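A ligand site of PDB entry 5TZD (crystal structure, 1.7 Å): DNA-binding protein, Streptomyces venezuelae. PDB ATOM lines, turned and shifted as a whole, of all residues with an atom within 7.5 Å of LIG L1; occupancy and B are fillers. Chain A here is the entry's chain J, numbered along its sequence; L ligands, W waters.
The backbone NH of Gln 51 sits at hydrogen-bond distance from an oxygen (O1) of LIG L1 (2.6 Å). The guanidinium group (NH2) of Arg 50 lies within hydrogen-bond range of an oxygen (O7) of LIG L1 (2.8 Å). NZ of Lys 9 lies within hydrogen-bond range of O6 of LIG L1, at 3.1 Å. The guanidinium group (NH2) of Arg 39 sits close to a nitrogen (N5) of LIG L1 (3.5 Å). An oxygen (O6) of LIG L1 is in hydrogen-bond range of the side-chain hydroxyl of Ser 48 (3.2 Å). The guanidinium group (NH2) of Arg 50 lies within salt-bridge range of an oxygen (O2) of LG2 L2 (3.0 Å). O14 of LG2 L2 is in hydrogen-bond range of NH2 of Arg 39. OD1 of Asp 53 is in hydrogen-bond range of N9 of LG2 L2 (2.7 Å).
A nitrogen (N3) of LIG L1 is in hydrogen-bond range of an oxygen (O9) of LG2 L2, 2.9 Å away.
The backbone NH (N) of Arg 50 sits at hydrogen-bond distance from the side-chain carboxylate (OD2) of Asp 53 (2.8 Å). The backbone carbonyl oxygen (O) of Ser 48 lies within hydrogen-bond range of the guanidinium group (NH2) of Arg 39 (2.9 Å). N of Ile 49 lies within hydrogen-bond range of O of Leu 10 (3.0 Å).
Residues that only touch LIG L1: Ile 49 (3.2 Å). Of the 14 residues printed, 6 come within 4 Å of LIG L1.
Water W3 lies within hydrogen-bond range of O9 of LIG L1 (2.5 Å) and N4 of LG2 L2 (3.4 Å). Water W10 lies within hydrogen-bond range of the backbone carbonyl oxygen of Ile 49 (2.8 Å) and the backbone NH of Leu 10 (2.9 Å). Water W1 bridges O9 of LG2 L2 (2.8 Å) and N4 of LIG L1 (3.2 Å). Water W5 bridges OG of Ser 48 (2.8 Å) and O6 of LIG L1 (3.4 Å).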
ATOM      1  N   LYS A   9      -8.240 -22.804   1.946  1.00  0.00           N
ATOM      2  CA  LYS A   9      -8.724 -23.098   0.601  1.00  0.00           C
ATOM      3  C   LYS A   9     -10.031 -23.906   0.600  1.00  0.00           C
ATOM      4  O   LYS A   9     -10.125 -24.959   1.232  1.00  0.00           O
ATOM      5  CB  LYS A   9      -7.660 -23.852  -0.187  1.00  0.00           C
ATOM      6  CG  LYS A   9      -7.658 -23.522  -1.673  1.00  0.00           C
ATOM      7  CD  LYS A   9      -7.499 -22.031  -1.901  1.00  0.00           C
ATOM      8  CE  LYS A   9      -6.732 -21.721  -3.186  1.00  0.00           C
ATOM      9  NZ  LYS A   9      -7.368 -22.310  -4.382  1.00  0.00           N
ATOM     10  N   LEU A  10     -11.030 -23.380  -0.100  1.00  0.00           N
ATOM     11  CA  LEU A  10     -12.335 -24.008  -0.238  1.00  0.00           C
ATOM     12  C   LEU A  10     -12.360 -24.615  -1.614  1.00  0.00           C
ATOM     13  O   LEU A  10     -12.480 -23.895  -2.598  1.00  0.00           O
ATOM     14  CB  LEU A  10     -13.433 -22.937  -0.167  1.00  0.00           C
ATOM     15  CG  LEU A  10     -13.495 -22.226   1.175  1.00  0.00           C
ATOM     16  CD1 LEU A  10     -14.466 -21.057   1.085  1.00  0.00           C
ATOM     17  CD2 LEU A  10     -13.894 -23.216   2.270  1.00  0.00           C
ATOM     18  N   VAL A  11     -12.225 -25.939  -1.706  1.00  0.00           N
ATOM     19  CA  VAL A  11     -12.171 -26.613  -2.987  1.00  0.00           C
ATOM     20  C   VAL A  11     -13.309 -27.630  -3.096  1.00  0.00           C
ATOM     21  O   VAL A  11     -13.464 -28.494  -2.219  1.00  0.00           O
ATOM     22  CB  VAL A  11     -10.810 -27.321  -3.168  1.00  0.00           C
ATOM     23  CG1 VAL A  11     -10.742 -28.011  -4.528  1.00  0.00           C
ATOM     24  CG2 VAL A  11      -9.696 -26.293  -3.044  1.00  0.00           C
ATOM     25  N   ILE A  35     -19.515 -20.286 -11.844  1.00  0.00           N
ATOM     26  CA  ILE A  35     -18.135 -19.899 -11.600  1.00  0.00           C
ATOM     27  C   ILE A  35     -17.234 -20.622 -12.565  1.00  0.00           C
ATOM     28  O   ILE A  35     -16.375 -20.007 -13.171  1.00  0.00           O
ATOM     29  CB  ILE A  35     -17.694 -20.225 -10.178  1.00  0.00           C
ATOM     30  CG1 ILE A  35     -18.468 -19.328  -9.214  1.00  0.00           C
ATOM     31  CG2 ILE A  35     -16.132 -20.086 -10.059  1.00  0.00           C
ATOM     32  CD1 ILE A  35     -18.201 -19.664  -7.768  1.00  0.00           C
ATOM     33  N   GLN A  38     -17.623 -18.951 -16.021  1.00  0.00           N
ATOM     34  CA  GLN A  38     -17.074 -17.595 -16.040  1.00  0.00           C
ATOM     35  C   GLN A  38     -15.566 -17.578 -16.099  1.00  0.00           C
ATOM     36  O   GLN A  38     -14.975 -16.679 -16.701  1.00  0.00           O
ATOM     37  CB  GLN A  38     -17.525 -16.838 -14.798  1.00  0.00           C
ATOM     38  CG  GLN A  38     -19.016 -16.499 -14.793  1.00  0.00           C
ATOM     39  CD  GLN A  38     -19.436 -15.942 -13.448  1.00  0.00           C
ATOM     40  OE1 GLN A  38     -19.014 -16.439 -12.400  1.00  0.00           O
ATOM     41  NE2 GLN A  38     -20.271 -14.939 -13.456  1.00  0.00           N
ATOM     42  N   ARG A  39     -14.930 -18.559 -15.460  1.00  0.00           N
ATOM     43  CA  ARG A  39     -13.485 -18.723 -15.548  1.00  0.00           C
ATOM     44  C   ARG A  39     -13.008 -19.387 -16.818  1.00  0.00           C
ATOM     45  O   ARG A  39     -11.794 -19.387 -17.089  1.00  0.00           O
ATOM     46  CB  ARG A  39     -12.950 -19.562 -14.395  1.00  0.00           C
ATOM     47  CG  ARG A  39     -13.268 -18.985 -13.033  1.00  0.00           C
ATOM     48  CD  ARG A  39     -12.667 -19.865 -11.945  1.00  0.00           C
ATOM     49  NE  ARG A  39     -12.908 -19.384 -10.597  1.00  0.00           N
ATOM     50  CZ  ARG A  39     -12.515 -20.031  -9.509  1.00  0.00           C
ATOM     51  NH1 ARG A  39     -11.855 -21.178  -9.627  1.00  0.00           N
ATOM     52  NH2 ARG A  39     -12.776 -19.550  -8.312  1.00  0.00           N
ATOM     53  N   ASP A  41     -13.118 -22.626 -17.253  1.00  0.00           N
ATOM     54  CA  ASP A  41     -12.531 -23.909 -16.829  1.00  0.00           C
ATOM     55  C   ASP A  41     -13.469 -25.099 -17.103  1.00  0.00           C
ATOM     56  O   ASP A  41     -13.711 -25.948 -16.220  1.00  0.00           O
ATOM     57  CB  ASP A  41     -12.148 -23.831 -15.348  1.00  0.00           C
ATOM     58  CG  ASP A  41     -11.197 -24.930 -14.902  1.00  0.00           C
ATOM     59  OD1 ASP A  41     -10.519 -25.570 -15.756  1.00  0.00           O
ATOM     60  OD2 ASP A  41     -11.100 -25.132 -13.674  1.00  0.00           O
ATOM     61  N   LEU A  47     -13.070 -27.299  -8.087  1.00  0.00           N
ATOM     62  CA  LEU A  47     -13.289 -25.849  -8.280  1.00  0.00           C
ATOM     63  C   LEU A  47     -13.078 -25.138  -6.958  1.00  0.00           C
ATOM     64  O   LEU A  47     -13.825 -25.388  -6.012  1.00  0.00           O
ATOM     65  CB  LEU A  47     -14.728 -25.609  -8.738  1.00  0.00           C
ATOM     66  CG  LEU A  47     -15.075 -24.158  -9.051  1.00  0.00           C
ATOM     67  CD1 LEU A  47     -14.364 -23.688 -10.310  1.00  0.00           C
ATOM     68  CD2 LEU A  47     -16.605 -23.985  -9.181  1.00  0.00           C
ATOM     69  N   SER A  48     -12.041 -24.319  -6.879  1.00  0.00           N
ATOM     70  CA  SER A  48     -11.814 -23.427  -5.722  1.00  0.00           C
ATOM     71  C   SER A  48     -12.879 -22.344  -5.767  1.00  0.00           C
ATOM     72  O   SER A  48     -13.286 -21.947  -6.845  1.00  0.00           O
ATOM     73  CB  SER A  48     -10.427 -22.800  -5.807  1.00  0.00           C
ATOM     74  OG  SER A  48     -10.245 -22.126  -7.050  1.00  0.00           O
ATOM     75  N   ILE A  49     -13.373 -21.879  -4.616  1.00  0.00           N
ATOM     76  CA  ILE A  49     -14.349 -20.772  -4.581  1.00  0.00           C
ATOM     77  C   ILE A  49     -13.911 -19.730  -3.572  1.00  0.00           C
ATOM     78  O   ILE A  49     -13.041 -19.973  -2.722  1.00  0.00           O
ATOM     79  CB  ILE A  49     -15.781 -21.276  -4.232  1.00  0.00           C
ATOM     80  CG1 ILE A  49     -15.805 -21.938  -2.864  1.00  0.00           C
ATOM     81  CG2 ILE A  49     -16.246 -22.245  -5.311  1.00  0.00           C
ATOM     82  CD1 ILE A  49     -17.188 -22.375  -2.423  1.00  0.00           C
ATOM     83  N   ARG A  50     -14.485 -18.530  -3.659  1.00  0.00           N
ATOM     84  CA  ARG A  50     -14.188 -17.470  -2.692  1.00  0.00           C
ATOM     85  C   ARG A  50     -14.797 -17.733  -1.328  1.00  0.00           C
ATOM     86  O   ARG A  50     -15.885 -18.292  -1.201  1.00  0.00           O
ATOM     87  CB  ARG A  50     -14.720 -16.128  -3.205  1.00  0.00           C
ATOM     88  CG  ARG A  50     -14.125 -15.769  -4.575  1.00  0.00           C
ATOM     89  CD  ARG A  50     -14.591 -14.403  -5.037  1.00  0.00           C
ATOM     90  NE  ARG A  50     -14.013 -14.135  -6.352  1.00  0.00           N
ATOM     91  CZ  ARG A  50     -14.332 -13.107  -7.118  1.00  0.00           C
ATOM     92  NH1 ARG A  50     -15.227 -12.214  -6.703  1.00  0.00           N
ATOM     93  NH2 ARG A  50     -13.731 -12.959  -8.308  1.00  0.00           N
ATOM     94  N   GLN A  51     -14.121 -17.296  -0.289  1.00  0.00           N
ATOM     95  CA  GLN A  51     -14.733 -17.275   1.031  1.00  0.00           C
ATOM     96  C   GLN A  51     -16.099 -16.585   0.982  1.00  0.00           C
ATOM     97  O   GLN A  51     -17.032 -17.088   1.601  1.00  0.00           O
ATOM     98  CB  GLN A  51     -13.810 -16.575   2.039  1.00  0.00           C
ATOM     99  CG  GLN A  51     -12.631 -17.435   2.529  1.00  0.00           C
ATOM    100  CD  GLN A  51     -13.002 -18.436   3.622  1.00  0.00           C
ATOM    101  OE1 GLN A  51     -12.418 -19.514   3.706  1.00  0.00           O
ATOM    102  NE2 GLN A  51     -13.966 -18.080   4.469  1.00  0.00           N
ATOM    103  N   ASP A  52     -16.225 -15.466   0.257  1.00  0.00           N
ATOM    104  CA  ASP A  52     -17.516 -14.769   0.167  1.00  0.00           C
ATOM    105  C   ASP A  52     -18.565 -15.684  -0.449  1.00  0.00           C
ATOM    106  O   ASP A  52     -19.753 -15.505  -0.219  1.00  0.00           O
ATOM    107  CB  ASP A  52     -17.423 -13.527  -0.722  1.00  0.00           C
ATOM    108  CG  ASP A  52     -16.489 -12.470  -0.162  1.00  0.00           C
ATOM    109  OD1 ASP A  52     -16.530 -12.205   1.059  1.00  0.00           O
ATOM    110  OD2 ASP A  52     -15.699 -11.912  -0.966  1.00  0.00           O
ATOM    111  N   ASP A  53     -18.140 -16.612  -1.291  1.00  0.00           N
ATOM    112  CA  ASP A  53     -19.077 -17.555  -1.900  1.00  0.00           C
ATOM    113  C   ASP A  53     -19.646 -18.533  -0.897  1.00  0.00           C
ATOM    114  O   ASP A  53     -20.792 -18.945  -1.019  1.00  0.00           O
ATOM    115  CB  ASP A  53     -18.418 -18.355  -3.017  1.00  0.00           C
ATOM    116  CG  ASP A  53     -18.051 -17.504  -4.191  1.00  0.00           C
ATOM    117  OD1 ASP A  53     -18.828 -16.594  -4.545  1.00  0.00           O
ATOM    118  OD2 ASP A  53     -16.959 -17.748  -4.737  1.00  0.00           O
HETATM  119  P1  LIG L   1     -10.890 -16.042  -2.041  1.00  0.00           P
HETATM  120  O1  LIG L   1     -11.660 -16.697  -0.902  1.00  0.00           O
HETATM  121  O2  LIG L   1     -11.552 -14.782  -2.475  1.00  0.00           O
HETATM  122  O3  LIG L   1     -10.716 -16.990  -3.237  1.00  0.00           O
HETATM  123  C1  LIG L   1     -10.307 -18.265  -2.999  1.00  0.00           C
HETATM  124  C2  LIG L   1      -9.696 -18.921  -4.212  1.00  0.00           C
HETATM  125  O4  LIG L   1     -10.624 -19.009  -5.279  1.00  0.00           O
HETATM  126  C3  LIG L   1      -8.513 -18.131  -4.789  1.00  0.00           C
HETATM  127  O5  LIG L   1      -7.296 -18.455  -4.122  1.00  0.00           O
HETATM  128  C4  LIG L   1      -8.591 -18.781  -6.047  1.00  0.00           C
HETATM  129  O6  LIG L   1      -7.976 -20.032  -6.332  1.00  0.00           O
HETATM  130  C5  LIG L   1      -9.950 -18.834  -6.488  1.00  0.00           C
HETATM  131  N1  LIG L   1     -10.657 -17.635  -7.061  1.00  0.00           N
HETATM  132  C6  LIG L   1     -11.476 -16.755  -6.492  1.00  0.00           C
HETATM  133  N2  LIG L   1     -11.914 -15.931  -7.311  1.00  0.00           N
HETATM  134  C7  LIG L   1     -11.448 -16.183  -8.538  1.00  0.00           C
HETATM  135  C8  LIG L   1     -11.578 -15.663  -9.815  1.00  0.00           C
HETATM  136  O7  LIG L   1     -12.308 -14.592 -10.081  1.00  0.00           O
HETATM  137  N3  LIG L   1     -10.895 -16.251 -10.839  1.00  0.00           N
HETATM  138  C9  LIG L   1     -10.118 -17.355 -10.648  1.00  0.00           C
HETATM  139  N4  LIG L   1      -9.433 -17.929 -11.807  1.00  0.00           N
HETATM  140  N5  LIG L   1      -9.923 -17.900  -9.451  1.00  0.00           N
HETATM  141  C10 LIG L   1     -10.598 -17.354  -8.429  1.00  0.00           C
HETATM  142  P2  LIG L   1      -6.054 -17.456  -4.356  1.00  0.00           P
HETATM  143  O8  LIG L   1      -4.975 -18.229  -3.642  1.00  0.00           O
HETATM  144  O9  LIG L   1      -5.903 -17.251  -5.797  1.00  0.00           O
HETATM  145  O10 LIG L   1      -6.358 -16.136  -3.621  1.00  0.00           O
HETATM  146  C11 LIG L   1      -6.483 -16.208  -2.218  1.00  0.00           C
HETATM  147  C12 LIG L   1      -7.245 -15.047  -1.631  1.00  0.00           C
HETATM  148  O11 LIG L   1      -6.530 -13.786  -1.957  1.00  0.00           O
HETATM  149  C13 LIG L   1      -8.625 -14.866  -2.166  1.00  0.00           C
HETATM  150  O12 LIG L   1      -9.461 -15.681  -1.415  1.00  0.00           O
HETATM  151  C14 LIG L   1      -8.839 -13.407  -1.986  1.00  0.00           C
HETATM  152  O13 LIG L   1      -9.139 -13.023  -0.703  1.00  0.00           O
HETATM  153  C15 LIG L   1      -7.474 -12.822  -2.278  1.00  0.00           C
HETATM  154  N6  LIG L   1      -7.288 -12.428  -3.659  1.00  0.00           N
HETATM  155  C16 LIG L   1      -6.641 -13.040  -4.624  1.00  0.00           C
HETATM  156  N7  LIG L   1      -6.699 -12.412  -5.722  1.00  0.00           N
HETATM  157  C17 LIG L   1      -7.389 -11.289  -5.652  1.00  0.00           C
HETATM  158  C18 LIG L   1      -7.792 -10.193  -6.459  1.00  0.00           C
HETATM  159  O14 LIG L   1      -7.485 -10.083  -7.733  1.00  0.00           O
HETATM  160  N8  LIG L   1      -8.542  -9.203  -5.905  1.00  0.00           N
HETATM  161  C19 LIG L   1      -8.878  -9.248  -4.625  1.00  0.00           C
HETATM  162  N9  LIG L   1      -9.661  -8.231  -4.031  1.00  0.00           N
HETATM  163  N10 LIG L   1      -8.548 -10.240  -3.783  1.00  0.00           N
HETATM  164  C20 LIG L   1      -7.814 -11.245  -4.271  1.00  0.00           C
HETATM  165  P1  LG2 L   2     -13.682 -10.447 -11.591  1.00  0.00           P
HETATM  166  O1  LG2 L   2     -13.931  -9.048 -12.025  1.00  0.00           O
HETATM  167  O2  LG2 L   2     -14.111 -10.664 -10.188  1.00  0.00           O
HETATM  168  O3  LG2 L   2     -12.178 -10.913 -11.669  1.00  0.00           O
HETATM  169  C1  LG2 L   2     -11.583 -10.716 -12.904  1.00  0.00           C
HETATM  170  C2  LG2 L   2     -10.447 -11.702 -12.887  1.00  0.00           C
HETATM  171  O4  LG2 L   2      -9.441 -11.434 -12.006  1.00  0.00           O
HETATM  172  C3  LG2 L   2     -10.673 -13.155 -13.013  1.00  0.00           C
HETATM  173  O5  LG2 L   2     -11.036 -13.573 -14.290  1.00  0.00           O
HETATM  174  C4  LG2 L   2      -9.385 -13.650 -12.632  1.00  0.00           C
HETATM  175  O6  LG2 L   2      -8.409 -13.673 -13.703  1.00  0.00           O
HETATM  176  C5  LG2 L   2      -8.895 -12.680 -11.675  1.00  0.00           C
HETATM  177  N1  LG2 L   2      -9.251 -12.900 -10.237  1.00  0.00           N
HETATM  178  C6  LG2 L   2     -10.198 -12.332  -9.473  1.00  0.00           C
HETATM  179  N2  LG2 L   2     -10.149 -12.769  -8.307  1.00  0.00           N
HETATM  180  C7  LG2 L   2      -9.225 -13.693  -8.146  1.00  0.00           C
HETATM  181  C8  LG2 L   2      -8.727 -14.495  -7.139  1.00  0.00           C
HETATM  182  O7  LG2 L   2      -9.232 -14.474  -5.878  1.00  0.00           O
HETATM  183  N3  LG2 L   2      -7.700 -15.338  -7.384  1.00  0.00           N
HETATM  184  C9  LG2 L   2      -7.155 -15.442  -8.647  1.00  0.00           C
HETATM  185  N4  LG2 L   2      -6.054 -16.388  -8.860  1.00  0.00           N
HETATM  186  N5  LG2 L   2      -7.564 -14.668  -9.675  1.00  0.00           N
HETATM  187  C10 LG2 L   2      -8.571 -13.807  -9.445  1.00  0.00           C
HETATM  188  P2  LG2 L   2     -11.891 -14.867 -14.475  1.00  0.00           P
HETATM  189  O8  LG2 L   2     -12.057 -15.168 -15.953  1.00  0.00           O
HETATM  190  O9  LG2 L   2     -11.176 -15.935 -13.709  1.00  0.00           O
HETATM  191  O10 LG2 L   2     -13.301 -14.650 -13.780  1.00  0.00           O
HETATM  192  C11 LG2 L   2     -14.187 -13.830 -14.481  1.00  0.00           C
HETATM  193  C12 LG2 L   2     -15.161 -13.431 -13.415  1.00  0.00           C
HETATM  194  O11 LG2 L   2     -16.119 -14.477 -13.142  1.00  0.00           O
HETATM  195  C13 LG2 L   2     -14.781 -12.627 -12.246  1.00  0.00           C
HETATM  196  O12 LG2 L   2     -14.580 -11.254 -12.580  1.00  0.00           O
HETATM  197  C14 LG2 L   2     -15.948 -12.918 -11.378  1.00  0.00           C
HETATM  198  O13 LG2 L   2     -16.976 -12.035 -11.591  1.00  0.00           O
HETATM  199  C15 LG2 L   2     -16.377 -14.316 -11.788  1.00  0.00           C
HETATM  200  N6  LG2 L   2     -15.735 -15.382 -11.057  1.00  0.00           N
HETATM  201  C16 LG2 L   2     -14.730 -16.151 -11.359  1.00  0.00           C
HETATM  202  N7  LG2 L   2     -14.499 -16.954 -10.439  1.00  0.00           N
HETATM  203  C17 LG2 L   2     -15.238 -16.780  -9.353  1.00  0.00           C
HETATM  204  C18 LG2 L   2     -15.433 -17.330  -8.074  1.00  0.00           C
HETATM  205  O14 LG2 L   2     -14.714 -18.304  -7.584  1.00  0.00           O
HETATM  206  N8  LG2 L   2     -16.414 -16.856  -7.308  1.00  0.00           N
HETATM  207  C19 LG2 L   2     -17.197 -15.813  -7.689  1.00  0.00           C
HETATM  208  N9  LG2 L   2     -18.223 -15.319  -6.797  1.00  0.00           N
HETATM  209  N10 LG2 L   2     -17.091 -15.224  -8.902  1.00  0.00           N
HETATM  210  C20 LG2 L   2     -16.108 -15.715  -9.720  1.00  0.00           C
HETATM  211  O   HOH W   1      -9.441 -17.685 -14.956  1.00  0.00           O
HETATM  212  O   HOH W   2     -10.275 -18.949   0.516  1.00  0.00           O
HETATM  213  O   HOH W   3      -4.194 -18.619  -7.084  1.00  0.00           O
HETATM  214  O   HOH W   4     -10.477 -14.414   1.285  1.00  0.00           O
HETATM  215  O   HOH W   5      -7.738 -23.060  -7.857  1.00  0.00           O
HETATM  216  O   HOH W   6      -3.432 -18.839  -1.463  1.00  0.00           O
HETATM  217  O   HOH W   7     -11.677  -8.368  -1.385  1.00  0.00           O
HETATM  218  O   HOH W   8      -8.010 -20.024  -9.130  1.00  0.00           O
HETATM  219  O   HOH W   9      -9.737 -10.044  -0.399  1.00  0.00           O
HETATM  220  O   HOH W  10     -10.659 -20.784  -1.394  1.00  0.00           O
